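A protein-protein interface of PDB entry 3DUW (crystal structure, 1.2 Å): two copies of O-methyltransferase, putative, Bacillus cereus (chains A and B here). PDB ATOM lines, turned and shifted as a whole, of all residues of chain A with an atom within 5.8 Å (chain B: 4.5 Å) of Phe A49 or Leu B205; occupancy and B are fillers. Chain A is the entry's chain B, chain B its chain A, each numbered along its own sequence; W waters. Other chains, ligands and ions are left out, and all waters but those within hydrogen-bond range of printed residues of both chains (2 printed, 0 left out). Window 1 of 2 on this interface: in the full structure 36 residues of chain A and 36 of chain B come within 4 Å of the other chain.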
ATOM      1  N   VAL A  14     -18.709  -3.698 -14.985  1.00  0.00           N
ATOM      2  CA  VAL A  14     -17.695  -3.734 -13.937  1.00  0.00           C
ATOM      3  C   VAL A  14     -16.718  -2.568 -14.041  1.00  0.00           C
ATOM      4  O   VAL A  14     -16.436  -1.893 -13.052  1.00  0.00           O
ATOM      5  CB  VAL A  14     -16.913  -5.065 -13.978  1.00  0.00           C
ATOM      6  CG1 VAL A  14     -15.791  -5.047 -12.949  1.00  0.00           C
ATOM      7  CG2 VAL A  14     -17.861  -6.222 -13.709  1.00  0.00           C
ATOM      8  N   PRO A  44      -9.127  -4.328 -19.004  1.00  0.00           N
ATOM      9  CA  PRO A  44      -9.025  -3.374 -17.901  1.00  0.00           C
ATOM     10  C   PRO A  44      -9.245  -4.026 -16.530  1.00  0.00           C
ATOM     11  O   PRO A  44      -8.545  -3.708 -15.570  1.00  0.00           O
ATOM     12  CB  PRO A  44     -10.112  -2.351 -18.230  1.00  0.00           C
ATOM     13  CG  PRO A  44     -10.159  -2.371 -19.721  1.00  0.00           C
ATOM     14  CD  PRO A  44     -10.069  -3.848 -20.032  1.00  0.00           C
ATOM     15  N   THR A  45     -10.218  -4.929 -16.430  1.00  0.00           N
ATOM     16  CA  THR A  45     -10.489  -5.575 -15.148  1.00  0.00           C
ATOM     17  C   THR A  45      -9.355  -6.512 -14.740  1.00  0.00           C
ATOM     18  O   THR A  45      -9.060  -6.656 -13.550  1.00  0.00           O
ATOM     19  CB  THR A  45     -11.832  -6.345 -15.170  1.00  0.00           C
ATOM     20  OG1 THR A  45     -11.848  -7.250 -16.277  1.00  0.00           O
ATOM     21  CG2 THR A  45     -13.003  -5.375 -15.287  1.00  0.00           C
ATOM     22  N   GLN A  46      -8.722  -7.142 -15.728  1.00  0.00           N
ATOM     23  CA  GLN A  46      -7.596  -8.034 -15.476  1.00  0.00           C
ATOM     24  C   GLN A  46      -6.405  -7.181 -15.053  1.00  0.00           C
ATOM     25  O   GLN A  46      -5.643  -7.551 -14.157  1.00  0.00           O
ATOM     26  CB  GLN A  46      -7.247  -8.817 -16.741  1.00  0.00           C
ATOM     27  CG  GLN A  46      -8.268  -9.878 -17.100  1.00  0.00           C
ATOM     28  CD  GLN A  46      -8.018 -10.482 -18.468  1.00  0.00           C
ATOM     29  OE1 GLN A  46      -7.155 -10.023 -19.215  1.00  0.00           O
ATOM     30  NE2 GLN A  46      -8.782 -11.510 -18.808  1.00  0.00           N
ATOM     31  N   GLY A  47      -6.253  -6.035 -15.708  1.00  0.00           N
ATOM     32  CA  GLY A  47      -5.167  -5.138 -15.374  1.00  0.00           C
ATOM     33  C   GLY A  47      -5.308  -4.656 -13.944  1.00  0.00           C
ATOM     34  O   GLY A  47      -4.335  -4.629 -13.190  1.00  0.00           O
ATOM     35  N   LYS A  48      -6.519  -4.276 -13.550  1.00  0.00           N
ATOM     36  CA  LYS A  48      -6.703  -3.807 -12.187  1.00  0.00           C
ATOM     37  C   LYS A  48      -6.486  -4.936 -11.183  1.00  0.00           C
ATOM     38  O   LYS A  48      -6.011  -4.704 -10.072  1.00  0.00           O
ATOM     39  CB  LYS A  48      -8.082  -3.183 -11.999  1.00  0.00           C
ATOM     40  CG  LYS A  48      -8.179  -2.479 -10.661  1.00  0.00           C
ATOM     41  CD  LYS A  48      -9.333  -1.511 -10.576  1.00  0.00           C
ATOM     42  CE  LYS A  48      -9.269  -0.751  -9.260  1.00  0.00           C
ATOM     43  NZ  LYS A  48     -10.363   0.239  -9.139  1.00  0.00           N
ATOM     44  N   PHE A  49      -6.839  -6.158 -11.568  1.00  0.00           N
ATOM     45  CA  PHE A  49      -6.613  -7.297 -10.692  1.00  0.00           C
ATOM     46  C   PHE A  49      -5.113  -7.404 -10.423  1.00  0.00           C
ATOM     47  O   PHE A  49      -4.691  -7.597  -9.284  1.00  0.00           O
ATOM     48  CB  PHE A  49      -7.124  -8.583 -11.344  1.00  0.00           C
ATOM     49  CG  PHE A  49      -6.763  -9.829 -10.586  1.00  0.00           C
ATOM     50  CD1 PHE A  49      -5.584 -10.512 -10.862  1.00  0.00           C
ATOM     51  CD2 PHE A  49      -7.586 -10.303  -9.569  1.00  0.00           C
ATOM     52  CE1 PHE A  49      -5.228 -11.653 -10.134  1.00  0.00           C
ATOM     53  CE2 PHE A  49      -7.239 -11.440  -8.839  1.00  0.00           C
ATOM     54  CZ  PHE A  49      -6.062 -12.112  -9.123  1.00  0.00           C
ATOM     55  N   LEU A  50      -4.308  -7.276 -11.476  1.00  0.00           N
ATOM     56  CA  LEU A  50      -2.856  -7.351 -11.330  1.00  0.00           C
ATOM     57  C   LEU A  50      -2.333  -6.233 -10.428  1.00  0.00           C
ATOM     58  O   LEU A  50      -1.499  -6.469  -9.550  1.00  0.00           O
ATOM     59  CB  LEU A  50      -2.175  -7.272 -12.701  1.00  0.00           C
ATOM     60  CG  LEU A  50      -2.369  -8.480 -13.625  1.00  0.00           C
ATOM     61  CD1 LEU A  50      -1.774  -8.184 -14.995  1.00  0.00           C
ATOM     62  CD2 LEU A  50      -1.715  -9.711 -13.010  1.00  0.00           C
ATOM     63  N   GLN A  51      -2.826  -5.018 -10.642  1.00  0.00           N
ATOM     64  CA  GLN A  51      -2.397  -3.880  -9.836  1.00  0.00           C
ATOM     65  C   GLN A  51      -2.685  -4.136  -8.361  1.00  0.00           C
ATOM     66  O   GLN A  51      -1.820  -3.958  -7.498  1.00  0.00           O
ATOM     67  CB  GLN A  51      -3.127  -2.617 -10.292  1.00  0.00           C
ATOM     68  CG  GLN A  51      -2.693  -1.345  -9.589  1.00  0.00           C
ATOM     69  CD  GLN A  51      -3.460  -0.138 -10.090  1.00  0.00           C
ATOM     70  OE1 GLN A  51      -4.633   0.041  -9.771  1.00  0.00           O
ATOM     71  NE2 GLN A  51      -2.806   0.686 -10.895  1.00  0.00           N
ATOM     72  N   LEU A  52      -3.910  -4.557  -8.071  1.00  0.00           N
ATOM     73  CA  LEU A  52      -4.296  -4.828  -6.696  1.00  0.00           C
ATOM     74  C   LEU A  52      -3.500  -5.984  -6.098  1.00  0.00           C
ATOM     75  O   LEU A  52      -3.122  -5.933  -4.928  1.00  0.00           O
ATOM     76  CB  LEU A  52      -5.800  -5.110  -6.618  1.00  0.00           C
ATOM     77  CG  LEU A  52      -6.680  -3.898  -6.944  1.00  0.00           C
ATOM     78  CD1 LEU A  52      -8.142  -4.324  -6.992  1.00  0.00           C
ATOM     79  CD2 LEU A  52      -6.474  -2.812  -5.897  1.00  0.00           C
ATOM     80  N   LEU A  53      -3.230  -7.021  -6.886  1.00  0.00           N
ATOM     81  CA  LEU A  53      -2.464  -8.151  -6.361  1.00  0.00           C
ATOM     82  C   LEU A  53      -1.037  -7.702  -6.035  1.00  0.00           C
ATOM     83  O   LEU A  53      -0.448  -8.138  -5.044  1.00  0.00           O
ATOM     84  CB  LEU A  53      -2.438  -9.305  -7.362  1.00  0.00           C
ATOM     85  CG  LEU A  53      -1.983 -10.631  -6.745  1.00  0.00           C
ATOM     86  CD1 LEU A  53      -2.955 -11.055  -5.646  1.00  0.00           C
ATOM     87  CD2 LEU A  53      -1.916 -11.695  -7.825  1.00  0.00           C
ATOM     88  N   VAL A  54      -0.483  -6.828  -6.867  1.00  0.00           N
ATOM     89  CA  VAL A  54       0.853  -6.302  -6.623  1.00  0.00           C
ATOM     90  C   VAL A  54       0.837  -5.539  -5.293  1.00  0.00           C
ATOM     91  O   VAL A  54       1.758  -5.666  -4.481  1.00  0.00           O
ATOM     92  CB  VAL A  54       1.290  -5.353  -7.767  1.00  0.00           C
ATOM     93  CG1 VAL A  54       2.509  -4.539  -7.350  1.00  0.00           C
ATOM     94  CG2 VAL A  54       1.607  -6.167  -9.023  1.00  0.00           C
ATOM     95  N   ILE A 164       1.949 -15.168 -11.803  1.00  0.00           N
ATOM     96  CA  ILE A 164       0.671 -15.182 -12.508  1.00  0.00           C
ATOM     97  C   ILE A 164       0.958 -15.587 -13.949  1.00  0.00           C
ATOM     98  O   ILE A 164       1.832 -15.009 -14.602  1.00  0.00           O
ATOM     99  CB  ILE A 164      -0.003 -13.791 -12.532  1.00  0.00           C
ATOM    100  CG1 ILE A 164      -0.406 -13.370 -11.117  1.00  0.00           C
ATOM    101  CG2 ILE A 164      -1.231 -13.826 -13.442  1.00  0.00           C
ATOM    102  CD1 ILE A 164      -1.520 -14.215 -10.512  1.00  0.00           C
ATOM    103  N   LEU A 205      -8.003 -20.124 -12.235  1.00  0.00           N
ATOM    104  CA  LEU A 205      -9.395 -19.731 -12.361  1.00  0.00           C
ATOM    105  C   LEU A 205      -9.677 -19.514 -13.837  1.00  0.00           C
ATOM    106  O   LEU A 205      -8.864 -18.920 -14.554  1.00  0.00           O
ATOM    107  CB  LEU A 205      -9.678 -18.429 -11.603  1.00  0.00           C
ATOM    108  CG  LEU A 205      -9.536 -18.440 -10.081  1.00  0.00           C
ATOM    109  CD1 LEU A 205     -10.030 -17.114  -9.527  1.00  0.00           C
ATOM    110  CD2 LEU A 205     -10.346 -19.586  -9.490  1.00  0.00           C
ATOM    111  N   THR A 207     -11.727 -17.684 -16.624  1.00  0.00           N
ATOM    112  CA  THR A 207     -12.394 -16.390 -16.657  1.00  0.00           C
ATOM    113  C   THR A 207     -13.107 -16.137 -17.989  1.00  0.00           C
ATOM    114  O   THR A 207     -12.782 -16.742 -19.005  1.00  0.00           O
ATOM    115  CB  THR A 207     -11.344 -15.293 -16.392  1.00  0.00           C
ATOM    116  OG1 THR A 207     -10.365 -15.314 -17.443  1.00  0.00           O
ATOM    117  CG2 THR A 207     -10.659 -15.516 -15.048  1.00  0.00           C
ATOM    118  N   VAL A 208     -14.105 -15.262 -17.967  1.00  0.00           N
ATOM    119  CA  VAL A 208     -14.787 -14.849 -19.178  1.00  0.00           C
ATOM    120  C   VAL A 208     -14.858 -13.335 -19.111  1.00  0.00           C
ATOM    121  O   VAL A 208     -14.752 -12.753 -18.029  1.00  0.00           O
ATOM    122  CB  VAL A 208     -16.192 -15.460 -19.352  1.00  0.00           C
ATOM    123  CG1 VAL A 208     -16.081 -16.967 -19.535  1.00  0.00           C
ATOM    124  CG2 VAL A 208     -17.078 -15.125 -18.181  1.00  0.00           C
ATOM    125  N   PHE A 216      -6.352 -17.928 -15.848  1.00  0.00           N
ATOM    126  CA  PHE A 216      -5.007 -17.692 -15.356  1.00  0.00           C
ATOM    127  C   PHE A 216      -4.639 -18.573 -14.182  1.00  0.00           C
ATOM    128  O   PHE A 216      -5.498 -19.056 -13.436  1.00  0.00           O
ATOM    129  CB  PHE A 216      -4.837 -16.225 -14.933  1.00  0.00           C
ATOM    130  CG  PHE A 216      -5.618 -15.845 -13.692  1.00  0.00           C
ATOM    131  CD1 PHE A 216      -6.988 -15.604 -13.756  1.00  0.00           C
ATOM    132  CD2 PHE A 216      -4.977 -15.731 -12.461  1.00  0.00           C
ATOM    133  CE1 PHE A 216      -7.707 -15.250 -12.614  1.00  0.00           C
ATOM    134  CE2 PHE A 216      -5.687 -15.379 -11.312  1.00  0.00           C
ATOM    135  CZ  PHE A 216      -7.053 -15.137 -11.389  1.00  0.00           C
ATOM    136  N   MET A 218      -2.429 -18.773 -10.672  1.00  0.00           N
ATOM    137  CA  MET A 218      -1.849 -17.945  -9.624  1.00  0.00           C
ATOM    138  C   MET A 218      -1.082 -18.926  -8.752  1.00  0.00           C
ATOM    139  O   MET A 218      -1.659 -19.859  -8.190  1.00  0.00           O
ATOM    140  CB  MET A 218      -2.907 -17.217  -8.790  1.00  0.00           C
ATOM    141  CG  MET A 218      -2.282 -16.347  -7.695  1.00  0.00           C
ATOM    142  SD  MET A 218      -3.510 -15.115  -6.858  1.00  0.00           S
ATOM    143  CE  MET A 218      -4.254 -16.288  -5.511  1.00  0.00           C
ATOM    144  N   PHE B  49      -7.716 -20.526  -4.251  1.00  0.00           N
ATOM    145  CA  PHE B  49      -7.441 -19.139  -4.597  1.00  0.00           C
ATOM    146  C   PHE B  49      -7.485 -18.329  -3.300  1.00  0.00           C
ATOM    147  O   PHE B  49      -6.612 -17.499  -3.043  1.00  0.00           O
ATOM    148  CB  PHE B  49      -8.496 -18.605  -5.567  1.00  0.00           C
ATOM    149  CG  PHE B  49      -8.357 -17.137  -5.854  1.00  0.00           C
ATOM    150  CD1 PHE B  49      -7.432 -16.678  -6.786  1.00  0.00           C
ATOM    151  CD2 PHE B  49      -9.120 -16.209  -5.155  1.00  0.00           C
ATOM    152  CE1 PHE B  49      -7.270 -15.310  -7.015  1.00  0.00           C
ATOM    153  CE2 PHE B  49      -8.962 -14.841  -5.378  1.00  0.00           C
ATOM    154  CZ  PHE B  49      -8.035 -14.394  -6.309  1.00  0.00           C
ATOM    155  N   THR B 203     -11.853  -4.431  -8.236  1.00  0.00           N
ATOM    156  CA  THR B 203     -12.058  -4.948  -9.572  1.00  0.00           C
ATOM    157  C   THR B 203     -12.935  -6.177  -9.387  1.00  0.00           C
ATOM    158  O   THR B 203     -13.208  -6.600  -8.258  1.00  0.00           O
ATOM    159  CB  THR B 203     -10.748  -5.366 -10.280  1.00  0.00           C
ATOM    160  OG1 THR B 203     -11.046  -5.644 -11.656  1.00  0.00           O
ATOM    161  CG2 THR B 203     -10.135  -6.612  -9.637  1.00  0.00           C
ATOM    162  N   ALA B 204     -13.404  -6.732 -10.494  1.00  0.00           N
ATOM    163  CA  ALA B 204     -14.203  -7.946 -10.441  1.00  0.00           C
ATOM    164  C   ALA B 204     -13.860  -8.792 -11.650  1.00  0.00           C
ATOM    165  O   ALA B 204     -13.710  -8.272 -12.758  1.00  0.00           O
ATOM    166  CB  ALA B 204     -15.699  -7.624 -10.444  1.00  0.00           C
ATOM    167  N   LEU B 205     -13.704 -10.091 -11.431  1.00  0.00           N
ATOM    168  CA  LEU B 205     -13.426 -11.012 -12.521  1.00  0.00           C
ATOM    169  C   LEU B 205     -14.612 -11.957 -12.638  1.00  0.00           C
ATOM    170  O   LEU B 205     -15.170 -12.399 -11.631  1.00  0.00           O
ATOM    171  CB  LEU B 205     -12.150 -11.826 -12.264  1.00  0.00           C
ATOM    172  CG  LEU B 205     -10.817 -11.073 -12.200  1.00  0.00           C
ATOM    173  CD1 LEU B 205      -9.674 -12.070 -12.028  1.00  0.00           C
ATOM    174  CD2 LEU B 205     -10.618 -10.251 -13.468  1.00  0.00           C
ATOM    175  N   GLN B 206     -15.019 -12.233 -13.871  1.00  0.00           N
ATOM    176  CA  GLN B 206     -16.106 -13.165 -14.119  1.00  0.00           C
ATOM    177  C   GLN B 206     -15.419 -14.514 -14.245  1.00  0.00           C
ATOM    178  O   GLN B 206     -14.382 -14.627 -14.904  1.00  0.00           O
ATOM    179  CB  GLN B 206     -16.815 -12.847 -15.432  1.00  0.00           C
ATOM    180  CG  GLN B 206     -17.323 -11.428 -15.557  1.00  0.00           C
ATOM    181  CD  GLN B 206     -17.993 -11.199 -16.893  1.00  0.00           C
ATOM    182  OE1 GLN B 206     -18.951 -11.890 -17.240  1.00  0.00           O
ATOM    183  NE2 GLN B 206     -17.493 -10.239 -17.653  1.00  0.00           N
ATOM    184  N   THR B 207     -15.980 -15.537 -13.615  1.00  0.00           N
ATOM    185  CA  THR B 207     -15.381 -16.859 -13.682  1.00  0.00           C
ATOM    186  C   THR B 207     -16.374 -17.913 -14.120  1.00  0.00           C
ATOM    187  O   THR B 207     -17.587 -17.738 -13.999  1.00  0.00           O
ATOM    188  CB  THR B 207     -14.819 -17.312 -12.310  1.00  0.00           C
ATOM    189  OG1 THR B 207     -15.899 -17.520 -11.384  1.00  0.00           O
ATOM    190  CG2 THR B 207     -13.864 -16.267 -11.751  1.00  0.00           C
ATOM    191  N   ASP B 214     -20.203 -17.208 -12.915  1.00  0.00           N
ATOM    192  CA  ASP B 214     -20.364 -16.269 -11.809  1.00  0.00           C
ATOM    193  C   ASP B 214     -19.146 -15.345 -11.769  1.00  0.00           C
ATOM    194  O   ASP B 214     -18.618 -14.969 -12.811  1.00  0.00           O
ATOM    195  CB  ASP B 214     -20.502 -17.046 -10.490  1.00  0.00           C
ATOM    196  CG  ASP B 214     -21.374 -16.335  -9.467  1.00  0.00           C
ATOM    197  OD1 ASP B 214     -21.513 -15.091  -9.536  1.00  0.00           O
ATOM    198  OD2 ASP B 214     -21.909 -17.031  -8.575  1.00  0.00           O
ATOM    199  N   GLY B 215     -18.697 -14.980 -10.575  1.00  0.00           N
ATOM    200  CA  GLY B 215     -17.554 -14.093 -10.483  1.00  0.00           C
ATOM    201  C   GLY B 215     -17.365 -13.538  -9.087  1.00  0.00           C
ATOM    202  O   GLY B 215     -18.195 -13.747  -8.205  1.00  0.00           O
ATOM    203  N   PHE B 216     -16.272 -12.811  -8.893  1.00  0.00           N
ATOM    204  CA  PHE B 216     -15.973 -12.240  -7.592  1.00  0.00           C
ATOM    205  C   PHE B 216     -15.359 -10.855  -7.665  1.00  0.00           C
ATOM    206  O   PHE B 216     -14.762 -10.462  -8.676  1.00  0.00           O
ATOM    207  CB  PHE B 216     -15.016 -13.150  -6.810  1.00  0.00           C
ATOM    208  CG  PHE B 216     -13.623 -13.207  -7.384  1.00  0.00           C
ATOM    209  CD1 PHE B 216     -13.343 -13.985  -8.506  1.00  0.00           C
ATOM    210  CD2 PHE B 216     -12.592 -12.469  -6.809  1.00  0.00           C
ATOM    211  CE1 PHE B 216     -12.054 -14.028  -9.047  1.00  0.00           C
ATOM    212  CE2 PHE B 216     -11.302 -12.505  -7.339  1.00  0.00           C
ATOM    213  CZ  PHE B 216     -11.035 -13.287  -8.460  1.00  0.00           C
ATOM    214  N   MET B 218     -12.696  -8.218  -5.808  1.00  0.00           N
ATOM    215  CA  MET B 218     -11.519  -8.181  -4.952  1.00  0.00           C
ATOM    216  C   MET B 218     -11.271  -6.699  -4.738  1.00  0.00           C
ATOM    217  O   MET B 218     -11.075  -5.945  -5.695  1.00  0.00           O
ATOM    218  CB  MET B 218     -10.298  -8.841  -5.602  1.00  0.00           C
ATOM    219  CG  MET B 218      -9.067  -8.814  -4.696  1.00  0.00           C
ATOM    220  SD  MET B 218      -7.603  -9.923  -5.296  1.00  0.00           S
ATOM    221  CE  MET B 218      -6.777  -8.666  -6.507  1.00  0.00           C
HETATM  222  O   HOH W   1     -13.650  -9.072 -15.491  1.00  0.00           O
HETATM  223  O   HOH W   2     -13.362 -11.568 -16.061  1.00  0.00           O
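The side-chain hydroxyl of Thr B203 is in hydrogen-bond range of the backbone carbonyl oxygen of Thr A45 (2.9 Å). O of Gln B206 sits at hydrogen-bond distance from N of Val A208, at 3.1 Å.
Among the printed residues, pairs that only touch across the chains: Thr A207 with Gln B206, Met A218 with Phe B49, Phe A49 with Met B218, Leu A52 with Met B218, Val A14 with Ala B204, Thr A45 with Ala B204, Phe A49 with Leu B205, Leu A205 with Phe B216, Phe A49 with Thr B203, Phe A216 with Leu B205, Leu A205 with Phe B49, Lys A48 with Thr B203, Leu A52 with Thr B203, Thr A45 with Leu B205, Leu A53 with Met B218 and Phe A49 with Phe B49.
Water W1 bridges the side-chain hydroxyl of Thr A45 (2.7 Å) and the backbone carbonyl oxygen of Ala B204 (2.8 Å). Water W2 lies within hydrogen-bond range of the backbone carbonyl oxygen (O) of Val A208 (2.7 Å) and the backbone NH (N) of Gln B206 (2.8 Å).
Phe A49 touches its own counterpart, Phe B49. Phe A49 touches Leu B205, and with the chains exchanged Leu A205 touches Phe B49. Phe A49 touches Met B218, and with the chains exchanged Met A218 touches Phe B49. Leu A205 touches Phe B216, and with the chains exchanged Phe A216 touches Leu B205. Positions printed for both chains: 49, 205, 207, 216 and 218.
The backbone carbonyl oxygen (O) of Phe B216 sits at hydrogen-bond distance from the backbone NH (N) of Leu B205 (3.0 Å). O of Phe A216 lies within hydrogen-bond range of N of Leu A205 (3.0 Å). The backbone NH of Met B218 lies within hydrogen-bond range of the backbone carbonyl oxygen of Thr B203.
Printed residues of chain B that touch a printed residue of chain A: Phe B49, Thr B203, Ala B204, Leu B205, Gln B206, Phe B216 and Met B218. Of the 18 printed residues of chain A, 11 touch a printed residue of chain B. Hydrophobic or aromatic side chains of chain A within 4 Å of the printed part of chain B: Val A14, Phe A49, Leu A52, Leu A205, Val A208, Phe A216 and Met A218.
Printed residues of chain B within 4 Å of Thr A45: Thr B203 (2.9 Å), Ala B204 (3.6 Å) and Leu B205 (3.9 Å). Printed residues of chain B within 4 Å of Phe A49: Phe B49 (3.97 Å), Thr B203 (3.7 Å), Leu B205 (3.7 Å) and Met B218 (3.6 Å). Printed residues of chain B within 4 Å of Leu A52: Thr B203 and Met B218. Of the printed residues of chain B, Thr A207 touches Gln B206 (3.2 Å). Printed residues of chain A within 4 Å of Leu B205: Thr A45 (3.9 Å), Phe A49 (3.7 Å) and Phe A216 (3.8 Å). Thr B207 touches none of the printed residues of chain A.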
